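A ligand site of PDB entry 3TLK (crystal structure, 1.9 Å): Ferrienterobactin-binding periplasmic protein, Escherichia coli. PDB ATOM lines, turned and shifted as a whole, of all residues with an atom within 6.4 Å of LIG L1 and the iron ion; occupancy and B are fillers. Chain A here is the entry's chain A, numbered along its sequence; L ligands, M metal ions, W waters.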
ATOM      1  N   VAL A  54      24.999  -0.163 -17.030  1.00  0.00           N
ATOM      2  CA  VAL A  54      25.131   1.255 -16.718  1.00  0.00           C
ATOM      3  C   VAL A  54      25.974   1.464 -15.434  1.00  0.00           C
ATOM      4  O   VAL A  54      26.716   2.454 -15.317  1.00  0.00           O
ATOM      5  CB  VAL A  54      23.768   1.973 -16.684  1.00  0.00           C
ATOM      6  CG1 VAL A  54      22.967   1.574 -15.435  1.00  0.00           C
ATOM      7  CG2 VAL A  54      23.954   3.484 -16.757  1.00  0.00           C
ATOM      8  N   THR A  55      25.901   0.538 -14.485  1.00  0.00           N
ATOM      9  CA  THR A  55      26.734   0.625 -13.276  1.00  0.00           C
ATOM     10  C   THR A  55      28.237   0.591 -13.595  1.00  0.00           C
ATOM     11  O   THR A  55      29.012   1.428 -13.108  1.00  0.00           O
ATOM     12  CB  THR A  55      26.419  -0.512 -12.250  1.00  0.00           C
ATOM     13  OG1 THR A  55      25.034  -0.473 -11.890  1.00  0.00           O
ATOM     14  CG2 THR A  55      27.251  -0.373 -10.969  1.00  0.00           C
ATOM     15  N   THR A  73      19.467   3.177 -18.077  1.00  0.00           N
ATOM     16  CA  THR A  73      18.186   2.924 -17.419  1.00  0.00           C
ATOM     17  C   THR A  73      17.203   3.978 -17.905  1.00  0.00           C
ATOM     18  O   THR A  73      17.468   4.659 -18.890  1.00  0.00           O
ATOM     19  CB  THR A  73      18.302   2.884 -15.868  1.00  0.00           C
ATOM     20  OG1 THR A  73      17.054   2.477 -15.297  1.00  0.00           O
ATOM     21  CG2 THR A  73      18.729   4.239 -15.315  1.00  0.00           C
ATOM     22  N   THR A  74      16.073   4.134 -17.232  1.00  0.00           N
ATOM     23  CA  THR A  74      15.046   5.059 -17.704  1.00  0.00           C
ATOM     24  C   THR A  74      15.432   6.530 -17.518  1.00  0.00           C
ATOM     25  O   THR A  74      15.714   6.954 -16.408  1.00  0.00           O
ATOM     26  CB  THR A  74      13.697   4.786 -16.978  1.00  0.00           C
ATOM     27  OG1 THR A  74      13.461   3.370 -16.928  1.00  0.00           O
ATOM     28  CG2 THR A  74      12.568   5.499 -17.682  1.00  0.00           C
ATOM     29  N   ASN A  77      14.497   9.025 -14.340  1.00  0.00           N
ATOM     30  CA  ASN A  77      14.010   8.289 -13.167  1.00  0.00           C
ATOM     31  C   ASN A  77      14.773   8.737 -11.920  1.00  0.00           C
ATOM     32  O   ASN A  77      15.491   9.734 -11.954  1.00  0.00           O
ATOM     33  CB  ASN A  77      14.029   6.756 -13.386  1.00  0.00           C
ATOM     34  CG  ASN A  77      15.409   6.139 -13.256  1.00  0.00           C
ATOM     35  OD1 ASN A  77      16.374   6.814 -12.933  1.00  0.00           O
ATOM     36  ND2 ASN A  77      15.498   4.833 -13.500  1.00  0.00           N
ATOM     37  N   ARG A  78      14.614   8.019 -10.822  1.00  0.00           N
ATOM     38  CA  ARG A  78      15.129   8.501  -9.546  1.00  0.00           C
ATOM     39  C   ARG A  78      16.652   8.608  -9.499  1.00  0.00           C
ATOM     40  O   ARG A  78      17.200   9.418  -8.730  1.00  0.00           O
ATOM     41  CB  ARG A  78      14.622   7.620  -8.406  1.00  0.00           C
ATOM     42  CG  ARG A  78      13.158   7.837  -8.064  1.00  0.00           C
ATOM     43  CD  ARG A  78      12.582   6.643  -7.287  1.00  0.00           C
ATOM     44  NE  ARG A  78      13.314   6.397  -6.047  1.00  0.00           N
ATOM     45  CZ  ARG A  78      13.196   5.292  -5.314  1.00  0.00           C
ATOM     46  NH1 ARG A  78      12.396   4.307  -5.694  1.00  0.00           N
ATOM     47  NH2 ARG A  78      13.905   5.158  -4.197  1.00  0.00           N
ATOM     48  N   VAL A  79      17.331   7.815 -10.323  1.00  0.00           N
ATOM     49  CA  VAL A  79      18.791   7.670 -10.236  1.00  0.00           C
ATOM     50  C   VAL A  79      19.549   8.086 -11.508  1.00  0.00           C
ATOM     51  O   VAL A  79      20.771   8.026 -11.555  1.00  0.00           O
ATOM     52  CB  VAL A  79      19.180   6.235  -9.851  1.00  0.00           C
ATOM     53  CG1 VAL A  79      18.543   5.860  -8.518  1.00  0.00           C
ATOM     54  CG2 VAL A  79      18.747   5.255 -10.941  1.00  0.00           C
ATOM     55  N   ALA A  80      18.820   8.545 -12.522  1.00  0.00           N
ATOM     56  CA  ALA A  80      19.442   8.789 -13.818  1.00  0.00           C
ATOM     57  C   ALA A  80      19.231  10.206 -14.350  1.00  0.00           C
ATOM     58  O   ALA A  80      18.340  10.927 -13.893  1.00  0.00           O
ATOM     59  CB  ALA A  80      18.958   7.756 -14.837  1.00  0.00           C
ATOM     60  N   LEU A  86      23.789   7.249 -15.156  1.00  0.00           N
ATOM     61  CA  LEU A  86      23.818   7.564 -13.720  1.00  0.00           C
ATOM     62  C   LEU A  86      24.314   8.982 -13.417  1.00  0.00           C
ATOM     63  O   LEU A  86      25.192   9.510 -14.102  1.00  0.00           O
ATOM     64  CB  LEU A  86      24.599   6.490 -12.938  1.00  0.00           C
ATOM     65  CG  LEU A  86      23.982   5.092 -13.034  1.00  0.00           C
ATOM     66  CD1 LEU A  86      24.860   4.086 -12.295  1.00  0.00           C
ATOM     67  CD2 LEU A  86      22.563   5.088 -12.434  1.00  0.00           C
ATOM     68  N   THR A 124      24.673  -9.203 -11.687  1.00  0.00           N
ATOM     69  CA  THR A 124      23.481  -8.974 -10.861  1.00  0.00           C
ATOM     70  C   THR A 124      22.967  -7.542 -11.075  1.00  0.00           C
ATOM     71  O   THR A 124      23.660  -6.741 -11.695  1.00  0.00           O
ATOM     72  CB  THR A 124      23.806  -9.140  -9.365  1.00  0.00           C
ATOM     73  OG1 THR A 124      24.775  -8.151  -8.970  1.00  0.00           O
ATOM     74  CG2 THR A 124      24.359 -10.533  -9.079  1.00  0.00           C
ATOM     75  N   GLY A 125      21.770  -7.247 -10.579  1.00  0.00           N
ATOM     76  CA  GLY A 125      21.184  -5.925 -10.699  1.00  0.00           C
ATOM     77  C   GLY A 125      20.240  -5.790 -11.882  1.00  0.00           C
ATOM     78  O   GLY A 125      20.206  -6.659 -12.768  1.00  0.00           O
ATOM     79  N   GLY A 126      19.473  -4.710 -11.913  1.00  0.00           N
ATOM     80  CA  GLY A 126      18.541  -4.437 -12.987  1.00  0.00           C
ATOM     81  C   GLY A 126      19.232  -4.182 -14.319  1.00  0.00           C
ATOM     82  O   GLY A 126      18.606  -4.255 -15.395  1.00  0.00           O
ATOM     83  N   ASP A 127      20.518  -3.865 -14.273  1.00  0.00           N
ATOM     84  CA  ASP A 127      21.276  -3.621 -15.510  1.00  0.00           C
ATOM     85  C   ASP A 127      22.031  -4.853 -16.025  1.00  0.00           C
ATOM     86  O   ASP A 127      22.850  -4.749 -16.946  1.00  0.00           O
ATOM     87  CB  ASP A 127      22.249  -2.446 -15.308  1.00  0.00           C
ATOM     88  CG  ASP A 127      23.206  -2.667 -14.174  1.00  0.00           C
ATOM     89  OD1 ASP A 127      22.997  -3.608 -13.375  1.00  0.00           O
ATOM     90  OD2 ASP A 127      24.179  -1.874 -14.053  1.00  0.00           O
ATOM     91  N   SER A 128      21.745  -6.030 -15.473  1.00  0.00           N
ATOM     92  CA  SER A 128      22.419  -7.248 -15.945  1.00  0.00           C
ATOM     93  C   SER A 128      21.862  -7.773 -17.284  1.00  0.00           C
ATOM     94  O   SER A 128      20.665  -8.070 -17.391  1.00  0.00           O
ATOM     95  CB  SER A 128      22.377  -8.368 -14.887  1.00  0.00           C
ATOM     96  OG  SER A 128      22.811  -9.600 -15.435  1.00  0.00           O
ATOM     97  N   TYR A 147      29.478  -6.462  -9.342  1.00  0.00           N
ATOM     98  CA  TYR A 147      29.702  -5.211  -8.593  1.00  0.00           C
ATOM     99  C   TYR A 147      29.027  -5.209  -7.223  1.00  0.00           C
ATOM    100  O   TYR A 147      29.170  -4.280  -6.452  1.00  0.00           O
ATOM    101  CB  TYR A 147      29.299  -3.978  -9.407  1.00  0.00           C
ATOM    102  CG  TYR A 147      27.830  -3.849  -9.769  1.00  0.00           C
ATOM    103  CD1 TYR A 147      26.886  -3.497  -8.811  1.00  0.00           C
ATOM    104  CD2 TYR A 147      27.394  -4.046 -11.086  1.00  0.00           C
ATOM    105  CE1 TYR A 147      25.545  -3.347  -9.143  1.00  0.00           C
ATOM    106  CE2 TYR A 147      26.056  -3.892 -11.426  1.00  0.00           C
ATOM    107  CZ  TYR A 147      25.141  -3.541 -10.444  1.00  0.00           C
ATOM    108  OH  TYR A 147      23.817  -3.396 -10.759  1.00  0.00           O
ATOM    109  N   VAL A 198      18.530   2.189   0.658  1.00  0.00           N
ATOM    110  CA  VAL A 198      17.853   3.027  -0.315  1.00  0.00           C
ATOM    111  C   VAL A 198      16.385   2.925   0.060  1.00  0.00           C
ATOM    112  O   VAL A 198      15.842   1.825   0.155  1.00  0.00           O
ATOM    113  CB  VAL A 198      18.015   2.503  -1.747  1.00  0.00           C
ATOM    114  CG1 VAL A 198      17.197   3.372  -2.729  1.00  0.00           C
ATOM    115  CG2 VAL A 198      19.484   2.511  -2.131  1.00  0.00           C
ATOM    116  N   TYR A 199      15.746   4.068   0.283  1.00  0.00           N
ATOM    117  CA  TYR A 199      14.365   4.102   0.727  1.00  0.00           C
ATOM    118  C   TYR A 199      13.458   4.437  -0.438  1.00  0.00           C
ATOM    119  O   TYR A 199      13.811   5.268  -1.263  1.00  0.00           O
ATOM    120  CB  TYR A 199      14.208   5.198   1.772  1.00  0.00           C
ATOM    121  CG  TYR A 199      12.839   5.299   2.433  1.00  0.00           C
ATOM    122  CD1 TYR A 199      12.319   4.207   3.117  1.00  0.00           C
ATOM    123  CD2 TYR A 199      12.116   6.500   2.421  1.00  0.00           C
ATOM    124  CE1 TYR A 199      11.097   4.297   3.753  1.00  0.00           C
ATOM    125  CE2 TYR A 199      10.885   6.590   3.041  1.00  0.00           C
ATOM    126  CZ  TYR A 199      10.387   5.494   3.721  1.00  0.00           C
ATOM    127  OH  TYR A 199       9.173   5.554   4.358  1.00  0.00           O
ATOM    128  N   THR A 200      12.288   3.803  -0.483  1.00  0.00           N
ATOM    129  CA  THR A 200      11.271   4.113  -1.492  1.00  0.00           C
ATOM    130  C   THR A 200      10.000   4.591  -0.794  1.00  0.00           C
ATOM    131  O   THR A 200       9.209   3.794  -0.299  1.00  0.00           O
ATOM    132  CB  THR A 200      10.994   2.931  -2.434  1.00  0.00           C
ATOM    133  OG1 THR A 200      12.166   2.670  -3.236  1.00  0.00           O
ATOM    134  CG2 THR A 200       9.837   3.261  -3.375  1.00  0.00           C
ATOM    135  N   ALA A 206      12.316  -0.534   1.848  1.00  0.00           N
ATOM    136  CA  ALA A 206      13.699  -0.150   1.623  1.00  0.00           C
ATOM    137  C   ALA A 206      14.517  -1.368   1.225  1.00  0.00           C
ATOM    138  O   ALA A 206      14.146  -2.503   1.510  1.00  0.00           O
ATOM    139  CB  ALA A 206      14.281   0.493   2.900  1.00  0.00           C
ATOM    140  N   ASN A 207      15.626  -1.128   0.547  1.00  0.00           N
ATOM    141  CA  ASN A 207      16.657  -2.130   0.408  1.00  0.00           C
ATOM    142  C   ASN A 207      17.851  -1.777   1.294  1.00  0.00           C
ATOM    143  O   ASN A 207      18.332  -0.657   1.277  1.00  0.00           O
ATOM    144  CB  ASN A 207      17.038  -2.315  -1.073  1.00  0.00           C
ATOM    145  CG  ASN A 207      15.887  -2.890  -1.870  1.00  0.00           C
ATOM    146  OD1 ASN A 207      15.356  -3.953  -1.512  1.00  0.00           O
ATOM    147  ND2 ASN A 207      15.484  -2.197  -2.926  1.00  0.00           N
ATOM    148  N   TRP A 209      21.672  -2.070   2.566  1.00  0.00           N
ATOM    149  CA  TRP A 209      22.983  -2.412   2.060  1.00  0.00           C
ATOM    150  C   TRP A 209      23.682  -3.344   3.032  1.00  0.00           C
ATOM    151  O   TRP A 209      23.629  -3.126   4.241  1.00  0.00           O
ATOM    152  CB  TRP A 209      23.847  -1.156   1.870  1.00  0.00           C
ATOM    153  CG  TRP A 209      23.321  -0.219   0.833  1.00  0.00           C
ATOM    154  CD1 TRP A 209      22.742   0.993   1.033  1.00  0.00           C
ATOM    155  CD2 TRP A 209      23.339  -0.433  -0.593  1.00  0.00           C
ATOM    156  NE1 TRP A 209      22.399   1.564  -0.176  1.00  0.00           N
ATOM    157  CE2 TRP A 209      22.748   0.712  -1.185  1.00  0.00           C
ATOM    158  CE3 TRP A 209      23.789  -1.466  -1.419  1.00  0.00           C
ATOM    159  CZ2 TRP A 209      22.621   0.839  -2.578  1.00  0.00           C
ATOM    160  CZ3 TRP A 209      23.645  -1.338  -2.784  1.00  0.00           C
ATOM    161  CH2 TRP A 209      23.065  -0.186  -3.355  1.00  0.00           C
ATOM    162  N   ARG A 242      22.307 -11.870  -5.689  1.00  0.00           N
ATOM    163  CA  ARG A 242      23.092 -10.693  -5.330  1.00  0.00           C
ATOM    164  C   ARG A 242      23.486 -10.652  -3.845  1.00  0.00           C
ATOM    165  O   ARG A 242      22.709 -11.066  -2.988  1.00  0.00           O
ATOM    166  CB  ARG A 242      22.343  -9.416  -5.711  1.00  0.00           C
ATOM    167  CG  ARG A 242      21.123  -9.138  -4.850  1.00  0.00           C
ATOM    168  CD  ARG A 242      20.171  -8.172  -5.544  1.00  0.00           C
ATOM    169  NE  ARG A 242      20.820  -6.900  -5.867  1.00  0.00           N
ATOM    170  CZ  ARG A 242      20.309  -5.975  -6.665  1.00  0.00           C
ATOM    171  NH1 ARG A 242      20.997  -4.837  -6.881  1.00  0.00           N
ATOM    172  NH2 ARG A 242      19.136  -6.165  -7.258  1.00  0.00           N
ATOM    173  N   ASP A 244      24.523  -7.649  -2.370  1.00  0.00           N
ATOM    174  CA  ASP A 244      24.584  -6.230  -1.980  1.00  0.00           C
ATOM    175  C   ASP A 244      23.437  -5.721  -1.093  1.00  0.00           C
ATOM    176  O   ASP A 244      23.626  -4.793  -0.327  1.00  0.00           O
ATOM    177  CB  ASP A 244      24.759  -5.328  -3.219  1.00  0.00           C
ATOM    178  CG  ASP A 244      23.713  -5.575  -4.312  1.00  0.00           C
ATOM    179  OD1 ASP A 244      23.014  -6.616  -4.316  1.00  0.00           O
ATOM    180  OD2 ASP A 244      23.609  -4.715  -5.215  1.00  0.00           O
ATOM    181  N   ILE A 245      22.265  -6.334  -1.188  1.00  0.00           N
ATOM    182  CA  ILE A 245      21.104  -5.827  -0.464  1.00  0.00           C
ATOM    183  C   ILE A 245      20.298  -6.952   0.163  1.00  0.00           C
ATOM    184  O   ILE A 245      20.412  -8.101  -0.221  1.00  0.00           O
ATOM    185  CB  ILE A 245      20.150  -5.021  -1.369  1.00  0.00           C
ATOM    186  CG1 ILE A 245      19.663  -5.872  -2.551  1.00  0.00           C
ATOM    187  CG2 ILE A 245      20.848  -3.752  -1.889  1.00  0.00           C
ATOM    188  CD1 ILE A 245      18.596  -5.203  -3.394  1.00  0.00           C
ATOM    189  N   PHE A 300      23.550   5.997  -5.727  1.00  0.00           N
ATOM    190  CA  PHE A 300      22.909   4.696  -5.977  1.00  0.00           C
ATOM    191  C   PHE A 300      23.964   3.627  -6.294  1.00  0.00           C
ATOM    192  O   PHE A 300      23.862   2.472  -5.877  1.00  0.00           O
ATOM    193  CB  PHE A 300      21.904   4.853  -7.140  1.00  0.00           C
ATOM    194  CG  PHE A 300      21.108   3.606  -7.443  1.00  0.00           C
ATOM    195  CD1 PHE A 300      20.274   3.028  -6.475  1.00  0.00           C
ATOM    196  CD2 PHE A 300      21.141   3.046  -8.709  1.00  0.00           C
ATOM    197  CE1 PHE A 300      19.531   1.893  -6.771  1.00  0.00           C
ATOM    198  CE2 PHE A 300      20.393   1.920  -9.015  1.00  0.00           C
ATOM    199  CZ  PHE A 300      19.589   1.337  -8.037  1.00  0.00           C
ATOM    200  N   ARG A 301      24.996   4.033  -7.032  1.00  0.00           N
ATOM    201  CA  ARG A 301      26.126   3.153  -7.319  1.00  0.00           C
ATOM    202  C   ARG A 301      27.399   3.899  -6.947  1.00  0.00           C
ATOM    203  O   ARG A 301      27.498   5.112  -7.145  1.00  0.00           O
ATOM    204  CB  ARG A 301      26.153   2.748  -8.799  1.00  0.00           C
ATOM    205  CG  ARG A 301      24.957   1.875  -9.248  1.00  0.00           C
ATOM    206  CD  ARG A 301      24.964   0.537  -8.515  1.00  0.00           C
ATOM    207  NE  ARG A 301      23.952  -0.409  -8.991  1.00  0.00           N
ATOM    208  CZ  ARG A 301      22.816  -0.681  -8.364  1.00  0.00           C
ATOM    209  NH1 ARG A 301      22.513  -0.040  -7.247  1.00  0.00           N
ATOM    210  NH2 ARG A 301      21.966  -1.602  -8.853  1.00  0.00           N
HETATM  211  O1  LIG L   1      19.714  -2.542  -7.712  1.00  0.00           O
HETATM  212  O2  LIG L   1      19.850  -2.562 -10.404  1.00  0.00           O
HETATM  213  O3  LIG L   1      18.146  -4.499  -9.180  1.00  0.00           O
HETATM  214  N1  LIG L   1      16.581   1.636 -10.842  1.00  0.00           N
HETATM  215  C1  LIG L   1      16.851  -4.932  -9.408  1.00  0.00           C
HETATM  216  C2  LIG L   1      19.843  -1.392 -11.148  1.00  0.00           C
HETATM  217  C3  LIG L   1      18.676  -0.382 -11.041  1.00  0.00           C
HETATM  218  C4  LIG L   1      15.802  -4.022  -9.634  1.00  0.00           C
HETATM  219  C5  LIG L   1      19.399  -1.962  -6.512  1.00  0.00           C
HETATM  220  C6  LIG L   1      16.538  -6.424  -9.333  1.00  0.00           C
HETATM  221  N2  LIG L   1      13.609  -2.144  -9.798  1.00  0.00           N
HETATM  222  C7  LIG L   1      20.424  -1.948  -5.375  1.00  0.00           C
HETATM  223  C8  LIG L   1      20.945   0.108 -12.861  1.00  0.00           C
HETATM  224  O4  LIG L   1      17.232  -1.443  -7.417  1.00  0.00           O
HETATM  225  N3  LIG L   1      15.767   0.286  -6.200  1.00  0.00           N
HETATM  226  C9  LIG L   1      18.714   0.800 -11.867  1.00  0.00           C
HETATM  227  C10 LIG L   1      20.923  -1.128 -12.019  1.00  0.00           C
HETATM  228  C11 LIG L   1      18.126  -1.338  -6.365  1.00  0.00           C
HETATM  229  C12 LIG L   1      15.226  -6.862  -9.487  1.00  0.00           C
HETATM  230  O5  LIG L   1      17.663  -0.600 -10.106  1.00  0.00           O
HETATM  231  O6  LIG L   1      16.103  -2.672  -9.772  1.00  0.00           O
HETATM  232  C13 LIG L   1      20.116  -1.303  -4.163  1.00  0.00           C
HETATM  233  C14 LIG L   1      18.815  -0.659  -3.995  1.00  0.00           C
HETATM  234  C15 LIG L   1      14.121  -5.906  -9.714  1.00  0.00           C
HETATM  235  C16 LIG L   1      19.836   1.060 -12.793  1.00  0.00           C
HETATM  236  O7  LIG L   1      17.406   2.614 -12.730  1.00  0.00           O
HETATM  237  C17 LIG L   1      17.582   1.802 -11.844  1.00  0.00           C
HETATM  238  C18 LIG L   1      15.408   2.443 -10.861  1.00  0.00           C
HETATM  239  C19 LIG L   1      14.942   2.733  -9.438  1.00  0.00           C
HETATM  240  O8  LIG L   1      14.851   3.962  -9.208  1.00  0.00           O
HETATM  241  O9  LIG L   1      15.317   2.027  -8.269  1.00  0.00           O
HETATM  242  C20 LIG L   1      15.064   2.558  -6.933  1.00  0.00           C
HETATM  243  C21 LIG L   1      14.708   1.250  -6.236  1.00  0.00           C
HETATM  244  C22 LIG L   1      16.494   0.024  -4.971  1.00  0.00           C
HETATM  245  C23 LIG L   1      17.809  -0.698  -5.123  1.00  0.00           C
HETATM  246  O10 LIG L   1      16.142   0.558  -3.929  1.00  0.00           O
HETATM  247  C24 LIG L   1      13.441   0.655  -6.843  1.00  0.00           C
HETATM  248  O11 LIG L   1      12.347   1.161  -6.460  1.00  0.00           O
HETATM  249  C25 LIG L   1      14.249   1.868 -11.674  1.00  0.00           C
HETATM  250  O12 LIG L   1      14.082   0.574 -11.103  1.00  0.00           O
HETATM  251  C26 LIG L   1      13.015   0.228 -10.267  1.00  0.00           C
HETATM  252  O13 LIG L   1      12.410   1.249  -9.777  1.00  0.00           O
HETATM  253  C27 LIG L   1      12.606  -1.111  -9.608  1.00  0.00           C
HETATM  254  C28 LIG L   1      12.042  -0.945  -8.169  1.00  0.00           C
HETATM  255  O14 LIG L   1      13.265  -0.594  -7.486  1.00  0.00           O
HETATM  256  C29 LIG L   1      13.282  -3.519  -9.935  1.00  0.00           C
HETATM  257  O15 LIG L   1      12.110  -3.860  -9.873  1.00  0.00           O
HETATM  258  C30 LIG L   1      14.417  -4.499  -9.802  1.00  0.00           C
HETATM  259  O1  LG2 L   2       8.685   3.713 -13.853  1.00  0.00           O
HETATM  260  O2  LG2 L   2       8.933   6.531 -12.442  1.00  0.00           O
HETATM  261  O3  LG2 L   2       5.958   5.637 -13.773  1.00  0.00           O
HETATM  262  N1  LG2 L   2       6.943   5.733  -7.635  1.00  0.00           N
HETATM  263  C1  LG2 L   2       4.655   5.343 -13.385  1.00  0.00           C
HETATM  264  C2  LG2 L   2       9.232   7.075 -11.182  1.00  0.00           C
HETATM  265  C3  LG2 L   2       8.474   6.581  -9.924  1.00  0.00           C
HETATM  266  C4  LG2 L   2       4.457   4.468 -12.310  1.00  0.00           C
HETATM  267  C5  LG2 L   2       9.238   2.510 -13.437  1.00  0.00           C
HETATM  268  C6  LG2 L   2       3.466   5.984 -14.079  1.00  0.00           C
HETATM  269  N2  LG2 L   2       4.036   2.539 -10.236  1.00  0.00           N
HETATM  270  C7  LG2 L   2      10.016   1.623 -14.420  1.00  0.00           C
HETATM  271  C8  LG2 L   2      10.553   8.605  -9.685  1.00  0.00           C
HETATM  272  O4  LG2 L   2       8.418   2.936 -11.203  1.00  0.00           O
HETATM  273  N3  LG2 L   2       9.130   1.337  -9.190  1.00  0.00           N
HETATM  274  C9  LG2 L   2       8.791   7.112  -8.615  1.00  0.00           C
HETATM  275  C10 LG2 L   2      10.230   8.063 -11.050  1.00  0.00           C
HETATM  276  C11 LG2 L   2       9.063   2.075 -12.076  1.00  0.00           C
HETATM  277  C12 LG2 L   2       2.174   5.714 -13.639  1.00  0.00           C
HETATM  278  O5  LG2 L   2       7.458   5.635 -10.091  1.00  0.00           O
HETATM  279  O6  LG2 L   2       5.579   3.875 -11.729  1.00  0.00           O
HETATM  280  C13 LG2 L   2      10.552   0.392 -13.990  1.00  0.00           C
HETATM  281  C14 LG2 L   2      10.375  -0.059 -12.602  1.00  0.00           C
HETATM  282  C15 LG2 L   2       1.953   4.798 -12.487  1.00  0.00           C
HETATM  283  C16 LG2 L   2       9.837   8.135  -8.469  1.00  0.00           C
HETATM  284  O7  LG2 L   2       8.484   6.695  -6.249  1.00  0.00           O
HETATM  285  C17 LG2 L   2       8.082   6.565  -7.399  1.00  0.00           C
HETATM  286  C18 LG2 L   2       6.479   5.009  -6.493  1.00  0.00           C
HETATM  287  C19 LG2 L   2       7.342   3.757  -6.230  1.00  0.00           C
HETATM  288  O8  LG2 L   2       6.796   2.954  -5.439  1.00  0.00           O
HETATM  289  O9  LG2 L   2       8.268   3.061  -7.090  1.00  0.00           O
HETATM  290  C20 LG2 L   2       8.855   1.796  -6.714  1.00  0.00           C
HETATM  291  C21 LG2 L   2       8.565   0.933  -7.948  1.00  0.00           C
HETATM  292  C22 LG2 L   2       9.365   0.333 -10.228  1.00  0.00           C
HETATM  293  C23 LG2 L   2       9.607   0.815 -11.644  1.00  0.00           C
HETATM  294  O10 LG2 L   2       9.479  -0.855  -9.901  1.00  0.00           O
HETATM  295  C24 LG2 L   2       7.102   0.536  -8.099  1.00  0.00           C
HETATM  296  O11 LG2 L   2       6.645   0.026  -7.041  1.00  0.00           O
HETATM  297  C25 LG2 L   2       4.977   4.782  -6.423  1.00  0.00           C
HETATM  298  O12 LG2 L   2       4.761   4.113  -7.672  1.00  0.00           O
HETATM  299  C26 LG2 L   2       4.139   2.838  -7.781  1.00  0.00           C
HETATM  300  O13 LG2 L   2       3.850   2.307  -6.648  1.00  0.00           O
HETATM  301  C27 LG2 L   2       3.933   1.871  -8.957  1.00  0.00           C
HETATM  302  C28 LG2 L   2       4.680   0.515  -8.760  1.00  0.00           C
HETATM  303  O14 LG2 L   2       6.058   0.907  -8.995  1.00  0.00           O
HETATM  304  C29 LG2 L   2       2.898   3.281 -10.654  1.00  0.00           C
HETATM  305  O15 LG2 L   2       1.876   3.239  -9.984  1.00  0.00           O
HETATM  306  C30 LG2 L   2       3.088   4.191 -11.835  1.00  0.00           C
HETATM  307 FE    FE M   1      18.130  -2.409  -9.093  1.00  0.00          FE
HETATM  308  O   HOH W   1      12.977   5.465 -10.603  1.00  0.00           O
HETATM  309  O   HOH W   2      14.131   1.050  -2.134  1.00  0.00           O
HETATM  310  O   HOH W   3      12.724   3.465 -13.923  1.00  0.00           O
HETATM  311  O   HOH W   4      16.807  -7.779  -6.244  1.00  0.00           O
HETATM  312  O   HOH W   5       9.771  -2.941  -8.286  1.00  0.00           O
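The side-chain hydroxyl (OG1) of Thr 55 lies within hydrogen-bond range of the side-chain carboxylate (OD2) of Asp 127. NH2 of Arg 301 is in hydrogen-bond range of OH of Tyr 147 (3.2 Å). OD1 of Asn 77 sits at hydrogen-bond distance from N of Val 79, 3.0 Å away. OD1 of Asp 127 sits at hydrogen-bond distance from OH of Tyr 147 (2.7 Å). The guanidinium group of Arg 78 lies within hydrogen-bond range of the backbone carbonyl oxygen of Tyr 199 (2.9 Å). OG1 of Thr 55 lies within hydrogen-bond range of NE of Arg 301 (3.1 Å). The side-chain hydroxyl (OH) of Tyr 147 lies within hydrogen-bond range of the side-chain hydroxyl (OG1) of Thr 55. The side-chain hydroxyl (OG1) of Thr 73 is in hydrogen-bond range of the side-chain amide nitrogen (ND2) of Asn 77 (3.3 Å).
Merely in contact with LIG L1: Val 198 (3.2 Å), Trp 209 (3.3 Å), Ile 245 (3.4 Å), Phe 300 (3.4 Å), Val 79 (3.5 Å), Asp 127 (3.5 Å), Thr 200 (3.6 Å), Gly 125 (3.6 Å), Val 54 (3.6 Å) and Tyr 147 (3.9 Å). Of the 26 residues printed, 17 come within 4 Å of LIG L1. The nearest printed residue that does not touch LIG L1 is Thr 55 (4.2 Å).
The iron ion is bound by O3 of LIG L1 (2.1 Å), O1 of LIG L1 (2.1 Å), O5 of LIG L1 (2.1 Å), O4 of LIG L1 (2.1 Å), O6 of LIG L1 (2.2 Å) and O2 of LIG L1 (2.2 Å).
An oxygen (O13) of LIG L1 lies close to a nitrogen (N3) of LG2 L2 (3.3 Å).
The guanidinium group (NH1) of Arg 78 lies within hydrogen-bond range of an oxygen (O11) of LIG L1 (3.2 Å). The side-chain hydroxyl (OG1) of Thr 73 is in hydrogen-bond range of an oxygen (O7) of LIG L1 (2.6 Å). The side-chain amide nitrogen (ND2) of Asn 77 is in hydrogen-bond range of an oxygen (O7) of LIG L1, at 3.0 Å. N of Gly 126 sits close to O2 of LIG L1 (2.7 Å). The guanidinium group (NH2) of Arg 242 sits close to an oxygen (O3) of LIG L1 (2.7 Å). The side-chain amide nitrogen of Asn 207 lies within hydrogen-bond range of an oxygen (O10) of LIG L1, 3.0 Å away. O1 of LIG L1 sits close to NH2 of Arg 301, 2.7 Å away.
Residues that only touch the iron ion: Gly 126 (3.9 Å) and Arg 301 (3.9 Å). The nearest printed residue that does not touch the iron ion is Phe 300 (4.2 Å).
Water W2 lies within hydrogen-bond range of O10 of LIG L1 (2.7 Å), OG1 of Thr 200 (2.8 Å) and O of Val 198 (3.0 Å). Water W1 bridges an oxygen (O8) of LIG L1 and the backbone NH of Arg 78. Water W5 lies within hydrogen-bond range of an oxygen (O10) of LG2 L2 (2.7 Å) and an oxygen (O15) of LIG L1 (3.0 Å). Water W3 lies within hydrogen-bond range of OG1 of Thr 74 (3.1 Å) and ND2 of Asn 77 (3.1 Å).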
